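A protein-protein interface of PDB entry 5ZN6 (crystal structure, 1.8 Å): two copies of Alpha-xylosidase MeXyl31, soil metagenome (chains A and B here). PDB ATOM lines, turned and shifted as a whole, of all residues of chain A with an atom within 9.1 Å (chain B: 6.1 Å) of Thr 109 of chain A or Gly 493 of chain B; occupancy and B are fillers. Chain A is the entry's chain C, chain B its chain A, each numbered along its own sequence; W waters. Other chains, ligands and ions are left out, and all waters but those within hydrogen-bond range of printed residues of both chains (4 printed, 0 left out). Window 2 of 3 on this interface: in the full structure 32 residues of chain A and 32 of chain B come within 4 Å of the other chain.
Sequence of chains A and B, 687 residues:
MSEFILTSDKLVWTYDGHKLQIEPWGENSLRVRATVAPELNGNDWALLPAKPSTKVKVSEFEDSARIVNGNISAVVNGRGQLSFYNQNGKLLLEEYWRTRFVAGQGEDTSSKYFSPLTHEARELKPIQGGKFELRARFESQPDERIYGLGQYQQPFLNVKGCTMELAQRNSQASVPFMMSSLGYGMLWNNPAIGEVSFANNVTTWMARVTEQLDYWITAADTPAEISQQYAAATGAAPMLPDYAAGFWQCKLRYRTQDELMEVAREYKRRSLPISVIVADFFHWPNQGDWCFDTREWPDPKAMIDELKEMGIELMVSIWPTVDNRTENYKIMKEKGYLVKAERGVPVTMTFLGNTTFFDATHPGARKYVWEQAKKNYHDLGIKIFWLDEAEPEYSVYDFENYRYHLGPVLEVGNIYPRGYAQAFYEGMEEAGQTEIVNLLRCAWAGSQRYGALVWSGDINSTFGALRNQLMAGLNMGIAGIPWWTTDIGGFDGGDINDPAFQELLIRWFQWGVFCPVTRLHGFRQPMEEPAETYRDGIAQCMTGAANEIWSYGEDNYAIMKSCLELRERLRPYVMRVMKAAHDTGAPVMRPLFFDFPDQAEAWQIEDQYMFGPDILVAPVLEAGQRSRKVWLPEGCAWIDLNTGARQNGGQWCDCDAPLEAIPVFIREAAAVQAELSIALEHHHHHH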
ATOM      1  N   ARG A  79      39.448 -23.856 -13.922  1.00  0.00           N
ATOM      2  CA  ARG A  79      38.281 -24.680 -13.670  1.00  0.00           C
ATOM      3  C   ARG A  79      38.635 -26.139 -13.319  1.00  0.00           C
ATOM      4  O   ARG A  79      37.742 -26.977 -13.230  1.00  0.00           O
ATOM      5  CB  ARG A  79      37.364 -24.640 -14.888  1.00  0.00           C
ATOM      6  CG  ARG A  79      36.803 -23.255 -15.183  1.00  0.00           C
ATOM      7  CD  ARG A  79      36.132 -23.243 -16.547  1.00  0.00           C
ATOM      8  NE  ARG A  79      35.446 -21.978 -16.822  1.00  0.00           N
ATOM      9  CZ  ARG A  79      35.910 -20.965 -17.564  1.00  0.00           C
ATOM     10  NH1 ARG A  79      37.111 -21.005 -18.158  1.00  0.00           N
ATOM     11  NH2 ARG A  79      35.156 -19.884 -17.722  1.00  0.00           N
ATOM     12  N   THR A  99      29.621 -29.391 -19.203  1.00  0.00           N
ATOM     13  CA  THR A  99      28.865 -28.692 -18.146  1.00  0.00           C
ATOM     14  C   THR A  99      28.643 -27.219 -18.534  1.00  0.00           C
ATOM     15  O   THR A  99      29.269 -26.716 -19.478  1.00  0.00           O
ATOM     16  CB  THR A  99      29.596 -28.674 -16.790  1.00  0.00           C
ATOM     17  OG1 THR A  99      30.591 -27.648 -16.815  1.00  0.00           O
ATOM     18  CG2 THR A  99      30.254 -29.999 -16.460  1.00  0.00           C
ATOM     19  N   ARG A 100      27.733 -26.554 -17.820  1.00  0.00           N
ATOM     20  CA  ARG A 100      27.572 -25.098 -17.913  1.00  0.00           C
ATOM     21  C   ARG A 100      28.253 -24.358 -16.763  1.00  0.00           C
ATOM     22  O   ARG A 100      28.444 -23.140 -16.834  1.00  0.00           O
ATOM     23  CB  ARG A 100      26.097 -24.740 -17.999  1.00  0.00           C
ATOM     24  CG  ARG A 100      25.479 -25.327 -19.242  1.00  0.00           C
ATOM     25  CD  ARG A 100      24.150 -24.693 -19.609  1.00  0.00           C
ATOM     26  NE  ARG A 100      23.105 -25.081 -18.695  1.00  0.00           N
ATOM     27  CZ  ARG A 100      21.793 -24.975 -18.932  1.00  0.00           C
ATOM     28  NH1 ARG A 100      21.315 -24.483 -20.079  1.00  0.00           N
ATOM     29  NH2 ARG A 100      20.947 -25.381 -17.995  1.00  0.00           N
ATOM     30  N   GLY A 106      31.195 -20.155 -14.353  1.00  0.00           N
ATOM     31  CA  GLY A 106      30.561 -20.412 -15.641  1.00  0.00           C
ATOM     32  C   GLY A 106      31.532 -21.057 -16.614  1.00  0.00           C
ATOM     33  O   GLY A 106      32.723 -20.722 -16.644  1.00  0.00           O
ATOM     34  N   GLU A 107      31.043 -22.001 -17.410  1.00  0.00           N
ATOM     35  CA  GLU A 107      31.878 -22.596 -18.453  1.00  0.00           C
ATOM     36  C   GLU A 107      31.933 -21.624 -19.635  1.00  0.00           C
ATOM     37  O   GLU A 107      31.068 -20.763 -19.799  1.00  0.00           O
ATOM     38  CB  GLU A 107      31.362 -23.996 -18.855  1.00  0.00           C
ATOM     39  CG  GLU A 107      32.176 -24.740 -19.911  1.00  0.00           C
ATOM     40  CD  GLU A 107      33.651 -24.916 -19.531  1.00  0.00           C
ATOM     41  OE1 GLU A 107      34.461 -24.029 -19.878  1.00  0.00           O
ATOM     42  OE2 GLU A 107      34.006 -25.925 -18.896  1.00  0.00           O
ATOM     43  N   ASP A 108      32.989 -21.752 -20.424  1.00  0.00           N
ATOM     44  CA  ASP A 108      33.225 -20.944 -21.602  1.00  0.00           C
ATOM     45  C   ASP A 108      32.352 -21.432 -22.743  1.00  0.00           C
ATOM     46  O   ASP A 108      32.564 -22.531 -23.255  1.00  0.00           O
ATOM     47  CB  ASP A 108      34.712 -21.074 -21.960  1.00  0.00           C
ATOM     48  CG  ASP A 108      35.140 -20.219 -23.127  1.00  0.00           C
ATOM     49  OD1 ASP A 108      34.308 -19.648 -23.863  1.00  0.00           O
ATOM     50  OD2 ASP A 108      36.378 -20.165 -23.321  1.00  0.00           O
ATOM     51  N   THR A 109      31.411 -20.592 -23.187  1.00  0.00           N
ATOM     52  CA  THR A 109      30.495 -20.969 -24.270  1.00  0.00           C
ATOM     53  C   THR A 109      31.160 -21.199 -25.629  1.00  0.00           C
ATOM     54  O   THR A 109      30.554 -21.807 -26.507  1.00  0.00           O
ATOM     55  CB  THR A 109      29.385 -19.918 -24.468  1.00  0.00           C
ATOM     56  OG1 THR A 109      29.985 -18.636 -24.656  1.00  0.00           O
ATOM     57  CG2 THR A 109      28.431 -19.903 -23.280  1.00  0.00           C
ATOM     58  N   SER A 110      32.384 -20.704 -25.823  1.00  0.00           N
ATOM     59  CA  SER A 110      33.129 -20.982 -27.053  1.00  0.00           C
ATOM     60  C   SER A 110      33.781 -22.379 -27.083  1.00  0.00           C
ATOM     61  O   SER A 110      34.286 -22.789 -28.130  1.00  0.00           O
ATOM     62  CB  SER A 110      34.192 -19.895 -27.287  1.00  0.00           C
ATOM     63  OG  SER A 110      35.303 -20.089 -26.427  1.00  0.00           O
ATOM     64  N   SER A 111      33.780 -23.099 -25.960  1.00  0.00           N
ATOM     65  CA  SER A 111      34.434 -24.419 -25.850  1.00  0.00           C
ATOM     66  C   SER A 111      33.439 -25.567 -26.049  1.00  0.00           C
ATOM     67  O   SER A 111      32.276 -25.467 -25.665  1.00  0.00           O
ATOM     68  CB  SER A 111      35.086 -24.557 -24.472  1.00  0.00           C
ATOM     69  OG  SER A 111      35.611 -25.855 -24.244  1.00  0.00           O
ATOM     70  N   LYS A 112      33.918 -26.660 -26.633  1.00  0.00           N
ATOM     71  CA  LYS A 112      33.162 -27.938 -26.674  1.00  0.00           C
ATOM     72  C   LYS A 112      32.797 -28.467 -25.265  1.00  0.00           C
ATOM     73  O   LYS A 112      31.922 -29.310 -25.127  1.00  0.00           O
ATOM     74  CB  LYS A 112      33.941 -29.008 -27.442  1.00  0.00           C
ATOM     75  CG  LYS A 112      35.271 -29.427 -26.809  1.00  0.00           C
ATOM     76  CD  LYS A 112      35.878 -30.608 -27.557  1.00  0.00           C
ATOM     77  CE  LYS A 112      37.132 -31.122 -26.885  1.00  0.00           C
ATOM     78  NZ  LYS A 112      38.136 -30.060 -26.669  1.00  0.00           N
ATOM     79  N   TYR A 113      33.493 -27.987 -24.237  1.00  0.00           N
ATOM     80  CA  TYR A 113      33.125 -28.269 -22.858  1.00  0.00           C
ATOM     81  C   TYR A 113      31.773 -27.685 -22.400  1.00  0.00           C
ATOM     82  O   TYR A 113      31.245 -28.120 -21.377  1.00  0.00           O
ATOM     83  CB  TYR A 113      34.226 -27.788 -21.903  1.00  0.00           C
ATOM     84  CG  TYR A 113      35.536 -28.580 -21.871  1.00  0.00           C
ATOM     85  CD1 TYR A 113      35.696 -29.828 -22.520  1.00  0.00           C
ATOM     86  CD2 TYR A 113      36.603 -28.106 -21.104  1.00  0.00           C
ATOM     87  CE1 TYR A 113      36.889 -30.530 -22.423  1.00  0.00           C
ATOM     88  CE2 TYR A 113      37.784 -28.812 -20.999  1.00  0.00           C
ATOM     89  CZ  TYR A 113      37.921 -30.015 -21.657  1.00  0.00           C
ATOM     90  OH  TYR A 113      39.093 -30.687 -21.530  1.00  0.00           O
ATOM     91  N   PHE A 114      31.221 -26.713 -23.132  1.00  0.00           N
ATOM     92  CA  PHE A 114      29.990 -26.073 -22.721  1.00  0.00           C
ATOM     93  C   PHE A 114      28.797 -26.900 -23.149  1.00  0.00           C
ATOM     94  O   PHE A 114      28.518 -27.018 -24.346  1.00  0.00           O
ATOM     95  CB  PHE A 114      29.838 -24.659 -23.278  1.00  0.00           C
ATOM     96  CG  PHE A 114      28.754 -23.888 -22.594  1.00  0.00           C
ATOM     97  CD1 PHE A 114      27.427 -24.043 -22.961  1.00  0.00           C
ATOM     98  CD2 PHE A 114      29.058 -23.047 -21.535  1.00  0.00           C
ATOM     99  CE1 PHE A 114      26.426 -23.358 -22.291  1.00  0.00           C
ATOM    100  CE2 PHE A 114      28.062 -22.359 -20.863  1.00  0.00           C
ATOM    101  CZ  PHE A 114      26.740 -22.513 -21.249  1.00  0.00           C
ATOM    102  N   SER A 115      28.071 -27.403 -22.159  1.00  0.00           N
ATOM    103  CA  SER A 115      26.940 -28.293 -22.387  1.00  0.00           C
ATOM    104  C   SER A 115      26.040 -28.378 -21.155  1.00  0.00           C
ATOM    105  O   SER A 115      26.537 -28.529 -20.038  1.00  0.00           O
ATOM    106  CB  SER A 115      27.449 -29.698 -22.733  1.00  0.00           C
ATOM    107  OG  SER A 115      26.400 -30.653 -22.740  1.00  0.00           O
ATOM    108  N   ILE B 459      22.201 -25.889 -26.681  1.00  0.00           N
ATOM    109  CA  ILE B 459      23.579 -26.050 -27.179  1.00  0.00           C
ATOM    110  C   ILE B 459      24.316 -24.716 -27.266  1.00  0.00           C
ATOM    111  O   ILE B 459      23.697 -23.652 -27.385  1.00  0.00           O
ATOM    112  CB  ILE B 459      23.572 -26.721 -28.565  1.00  0.00           C
ATOM    113  CG1 ILE B 459      22.678 -25.892 -29.539  1.00  0.00           C
ATOM    114  CG2 ILE B 459      23.096 -28.170 -28.407  1.00  0.00           C
ATOM    115  CD1 ILE B 459      22.427 -26.492 -30.874  1.00  0.00           C
ATOM    116  N   ASN B 460      25.641 -24.768 -27.213  1.00  0.00           N
ATOM    117  CA  ASN B 460      26.432 -23.560 -27.419  1.00  0.00           C
ATOM    118  C   ASN B 460      26.477 -23.113 -28.897  1.00  0.00           C
ATOM    119  O   ASN B 460      26.130 -23.865 -29.819  1.00  0.00           O
ATOM    120  CB  ASN B 460      27.828 -23.682 -26.799  1.00  0.00           C
ATOM    121  CG  ASN B 460      28.654 -24.812 -27.384  1.00  0.00           C
ATOM    122  OD1 ASN B 460      28.119 -25.783 -27.906  1.00  0.00           O
ATOM    123  ND2 ASN B 460      29.971 -24.695 -27.276  1.00  0.00           N
ATOM    124  N   SER B 461      26.871 -21.863 -29.103  1.00  0.00           N
ATOM    125  CA  SER B 461      26.896 -21.249 -30.426  1.00  0.00           C
ATOM    126  C   SER B 461      28.297 -21.388 -31.048  1.00  0.00           C
ATOM    127  O   SER B 461      29.087 -20.446 -31.029  1.00  0.00           O
ATOM    128  CB  SER B 461      26.450 -19.768 -30.344  1.00  0.00           C
ATOM    129  OG  SER B 461      25.068 -19.664 -30.050  1.00  0.00           O
ATOM    130  N   THR B 462      28.572 -22.569 -31.605  1.00  0.00           N
ATOM    131  CA  THR B 462      29.861 -22.881 -32.243  1.00  0.00           C
ATOM    132  C   THR B 462      29.643 -23.749 -33.462  1.00  0.00           C
ATOM    133  O   THR B 462      28.588 -24.391 -33.603  1.00  0.00           O
ATOM    134  CB  THR B 462      30.814 -23.659 -31.307  1.00  0.00           C
ATOM    135  OG1 THR B 462      30.244 -24.936 -30.989  1.00  0.00           O
ATOM    136  CG2 THR B 462      31.074 -22.895 -30.026  1.00  0.00           C
ATOM    137  N   PHE B 491      22.106 -21.853 -29.046  1.00  0.00           N
ATOM    138  CA  PHE B 491      21.436 -21.193 -27.929  1.00  0.00           C
ATOM    139  C   PHE B 491      22.333 -20.202 -27.191  1.00  0.00           C
ATOM    140  O   PHE B 491      21.974 -19.028 -27.063  1.00  0.00           O
ATOM    141  CB  PHE B 491      20.884 -22.230 -26.940  1.00  0.00           C
ATOM    142  CG  PHE B 491      20.210 -21.629 -25.721  1.00  0.00           C
ATOM    143  CD1 PHE B 491      18.968 -21.016 -25.820  1.00  0.00           C
ATOM    144  CD2 PHE B 491      20.825 -21.674 -24.483  1.00  0.00           C
ATOM    145  CE1 PHE B 491      18.346 -20.472 -24.704  1.00  0.00           C
ATOM    146  CE2 PHE B 491      20.226 -21.121 -23.359  1.00  0.00           C
ATOM    147  CZ  PHE B 491      18.967 -20.521 -23.469  1.00  0.00           C
ATOM    148  N   ASP B 492      23.477 -20.679 -26.705  1.00  0.00           N
ATOM    149  CA  ASP B 492      24.262 -19.985 -25.683  1.00  0.00           C
ATOM    150  C   ASP B 492      25.605 -19.482 -26.220  1.00  0.00           C
ATOM    151  O   ASP B 492      26.370 -20.263 -26.805  1.00  0.00           O
ATOM    152  CB  ASP B 492      24.528 -20.938 -24.498  1.00  0.00           C
ATOM    153  CG  ASP B 492      24.109 -20.357 -23.148  1.00  0.00           C
ATOM    154  OD1 ASP B 492      24.094 -19.115 -22.989  1.00  0.00           O
ATOM    155  OD2 ASP B 492      23.807 -21.157 -22.237  1.00  0.00           O
ATOM    156  N   GLY B 493      25.873 -18.189 -26.012  1.00  0.00           N
ATOM    157  CA  GLY B 493      27.204 -17.589 -26.230  1.00  0.00           C
ATOM    158  C   GLY B 493      27.411 -16.717 -27.451  1.00  0.00           C
ATOM    159  O   GLY B 493      28.504 -16.201 -27.639  1.00  0.00           O
ATOM    160  N   GLY B 494      26.401 -16.566 -28.299  1.00  0.00           N
ATOM    161  CA  GLY B 494      26.524 -15.710 -29.486  1.00  0.00           C
ATOM    162  C   GLY B 494      26.438 -14.206 -29.193  1.00  0.00           C
ATOM    163  O   GLY B 494      25.365 -13.709 -28.859  1.00  0.00           O
ATOM    164  N   ASP B 495      27.560 -13.490 -29.313  1.00  0.00           N
ATOM    165  CA  ASP B 495      27.562 -12.030 -29.219  1.00  0.00           C
ATOM    166  C   ASP B 495      27.133 -11.440 -30.569  1.00  0.00           C
ATOM    167  O   ASP B 495      27.758 -11.717 -31.603  1.00  0.00           O
ATOM    168  CB  ASP B 495      28.939 -11.491 -28.801  1.00  0.00           C
ATOM    169  CG  ASP B 495      28.914  -9.989 -28.520  1.00  0.00           C
ATOM    170  OD1 ASP B 495      28.586  -9.207 -29.426  1.00  0.00           O
ATOM    171  OD2 ASP B 495      29.167  -9.594 -27.370  1.00  0.00           O
ATOM    172  N   PHE B 501      30.779 -15.094 -34.503  1.00  0.00           N
ATOM    173  CA  PHE B 501      29.423 -15.601 -34.291  1.00  0.00           C
ATOM    174  C   PHE B 501      28.524 -15.319 -35.501  1.00  0.00           C
ATOM    175  O   PHE B 501      27.743 -16.190 -35.919  1.00  0.00           O
ATOM    176  CB  PHE B 501      28.763 -15.050 -33.011  1.00  0.00           C
ATOM    177  CG  PHE B 501      27.308 -15.426 -32.910  1.00  0.00           C
ATOM    178  CD1 PHE B 501      26.949 -16.770 -32.852  1.00  0.00           C
ATOM    179  CD2 PHE B 501      26.305 -14.466 -32.981  1.00  0.00           C
ATOM    180  CE1 PHE B 501      25.619 -17.150 -32.832  1.00  0.00           C
ATOM    181  CE2 PHE B 501      24.964 -14.835 -32.963  1.00  0.00           C
ATOM    182  CZ  PHE B 501      24.621 -16.184 -32.889  1.00  0.00           C
ATOM    183  N   PHE B 523      19.828 -17.199 -26.959  1.00  0.00           N
ATOM    184  CA  PHE B 523      20.076 -16.356 -25.814  1.00  0.00           C
ATOM    185  C   PHE B 523      21.344 -15.578 -26.148  1.00  0.00           C
ATOM    186  O   PHE B 523      22.452 -16.015 -25.849  1.00  0.00           O
ATOM    187  CB  PHE B 523      20.198 -17.212 -24.541  1.00  0.00           C
ATOM    188  CG  PHE B 523      20.631 -16.450 -23.326  1.00  0.00           C
ATOM    189  CD1 PHE B 523      20.166 -15.161 -23.082  1.00  0.00           C
ATOM    190  CD2 PHE B 523      21.504 -17.031 -22.411  1.00  0.00           C
ATOM    191  CE1 PHE B 523      20.586 -14.458 -21.966  1.00  0.00           C
ATOM    192  CE2 PHE B 523      21.925 -16.333 -21.293  1.00  0.00           C
ATOM    193  CZ  PHE B 523      21.467 -15.042 -21.067  1.00  0.00           C
ATOM    194  N   ARG B 524      21.163 -14.429 -26.796  1.00  0.00           N
ATOM    195  CA  ARG B 524      22.279 -13.681 -27.365  1.00  0.00           C
ATOM    196  C   ARG B 524      22.899 -12.744 -26.352  1.00  0.00           C
ATOM    197  O   ARG B 524      22.216 -12.219 -25.470  1.00  0.00           O
ATOM    198  CB  ARG B 524      21.809 -12.862 -28.565  1.00  0.00           C
ATOM    199  CG  ARG B 524      21.204 -13.673 -29.697  1.00  0.00           C
ATOM    200  CD  ARG B 524      22.176 -14.641 -30.373  1.00  0.00           C
ATOM    201  NE  ARG B 524      21.488 -15.221 -31.524  1.00  0.00           N
ATOM    202  CZ  ARG B 524      21.240 -16.513 -31.761  1.00  0.00           C
ATOM    203  NH1 ARG B 524      21.707 -17.495 -30.979  1.00  0.00           N
ATOM    204  NH2 ARG B 524      20.540 -16.830 -32.847  1.00  0.00           N
ATOM    205  N   GLN B 525      24.203 -12.533 -26.495  1.00  0.00           N
ATOM    206  CA  GLN B 525      24.966 -11.599 -25.671  1.00  0.00           C
ATOM    207  C   GLN B 525      25.091 -10.260 -26.428  1.00  0.00           C
ATOM    208  O   GLN B 525      25.011 -10.254 -27.658  1.00  0.00           O
ATOM    209  CB  GLN B 525      26.346 -12.189 -25.346  1.00  0.00           C
ATOM    210  CG  GLN B 525      26.292 -13.460 -24.501  1.00  0.00           C
ATOM    211  CD  GLN B 525      25.718 -13.237 -23.113  1.00  0.00           C
ATOM    212  OE1 GLN B 525      25.881 -12.168 -22.530  1.00  0.00           O
ATOM    213  NE2 GLN B 525      25.024 -14.244 -22.583  1.00  0.00           N
HETATM  214  O   HOH W   1      22.894 -23.704 -22.311  1.00  0.00           O
HETATM  215  O   HOH W   2      31.049 -17.820 -26.958  1.00  0.00           O
HETATM  216  O   HOH W   3      31.797 -26.386 -29.373  1.00  0.00           O
HETATM  217  O   HOH W   4      26.338 -27.815 -25.907  1.00  0.00           O
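The side-chain amide nitrogen (ND2) of Asn 460 of chain B sits at hydrogen-bond distance from the backbone carbonyl oxygen (O) of Thr 109 of chain A, 3.0 Å away. The backbone carbonyl oxygen (O) of Ser 111 of chain A lies within hydrogen-bond range of the side-chain amide nitrogen (ND2) of Asn 460 of chain B (2.9 Å).
O of Ile 459 of chain B is in hydrogen-bond range of N of Asp 492 of chain B. N of Ser 461 of chain B sits at hydrogen-bond distance from O of Asp 492 of chain B, 2.8 Å away. The side-chain carboxylate (OD1) of Asp 108 of chain A is in hydrogen-bond range of the side-chain hydroxyl (OG) of Ser 110 of chain A (2.8 Å). The backbone NH (N) of Tyr 113 of chain A lies within hydrogen-bond range of the side-chain hydroxyl (OG) of Ser 111 of chain A (3.0 Å).
Thr 109 of chain A touches Thr 462 of chain B. Asp 492 of chain B touches Thr 109 of chain A. Thr 109 of chain A touches Gly 493 of chain B (OG1 to CA, 3.4 Å). Thr 462 of chain B touches Ser 110 of chain A (CG2 to O, 3.7 Å). Asn 460 of chain B touches Phe 114 of chain A (CG to O, 3.8 Å). Phe 114 of chain A touches Asp 492 of chain B.
Thr 109 of chain A touches just these residues of chain B: Asn 460, Thr 462, Asp 492 and Gly 493. Of the printed residues of chain A, Gly 493 of chain B touches Thr 109 (3.4 Å). Asp 492 of chain B touches just these residues of chain A: Thr 109 (3.8 Å) and Phe 114 (3.4 Å). Printed residues of chain A within 4 Å of Thr 462 of chain B: Thr 109 (3.7 Å) and Ser 110 (3.7 Å). Of the printed residues of chain B, Phe 114 of chain A touches Asn 460 and Asp 492. Of the printed residues of chain B, Ser 110 of chain A touches Thr 462. Ser 115 of chain A touches none of the printed residues of chain B.
Of the 13 printed residues of chain A, 4 touch a printed residue of chain B. Printed residues of chain A that touch a printed residue of chain B: Thr 109, Ser 110, Ser 111 and Phe 114. Along chain A the printed residues that touch a printed residue of chain B span positions 109 to 114. Printed residues of chain B that touch a printed residue of chain A: Asn 460, Thr 462, Asp 492 and Gly 493.
No position is printed for both chains. Of the 8 pairs that touch across the chains among the printed residues, none has its exchanged pair printed and touching as well.
Water W2 lies within hydrogen-bond range of the side-chain hydroxyl of Thr 109 of chain A, the backbone carbonyl oxygen of Gly 493 of chain B and the backbone NH of Ser 110 of chain A. Water W3 lies within hydrogen-bond range of the side-chain hydroxyl of Thr 462 of chain B, the side-chain amide nitrogen of Asn 460 of chain B and the backbone NH of Lys 112 of chain A. Water W1 bridges OD2 of Asp 492 of chain B (2.7 Å) and NH1 of Arg 100 of chain A (2.8 Å). Water W4 bridges the backbone carbonyl oxygen (O) of Phe 114 of chain A and the side-chain amide oxygen (OD1) of Asn 460 of chain B.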
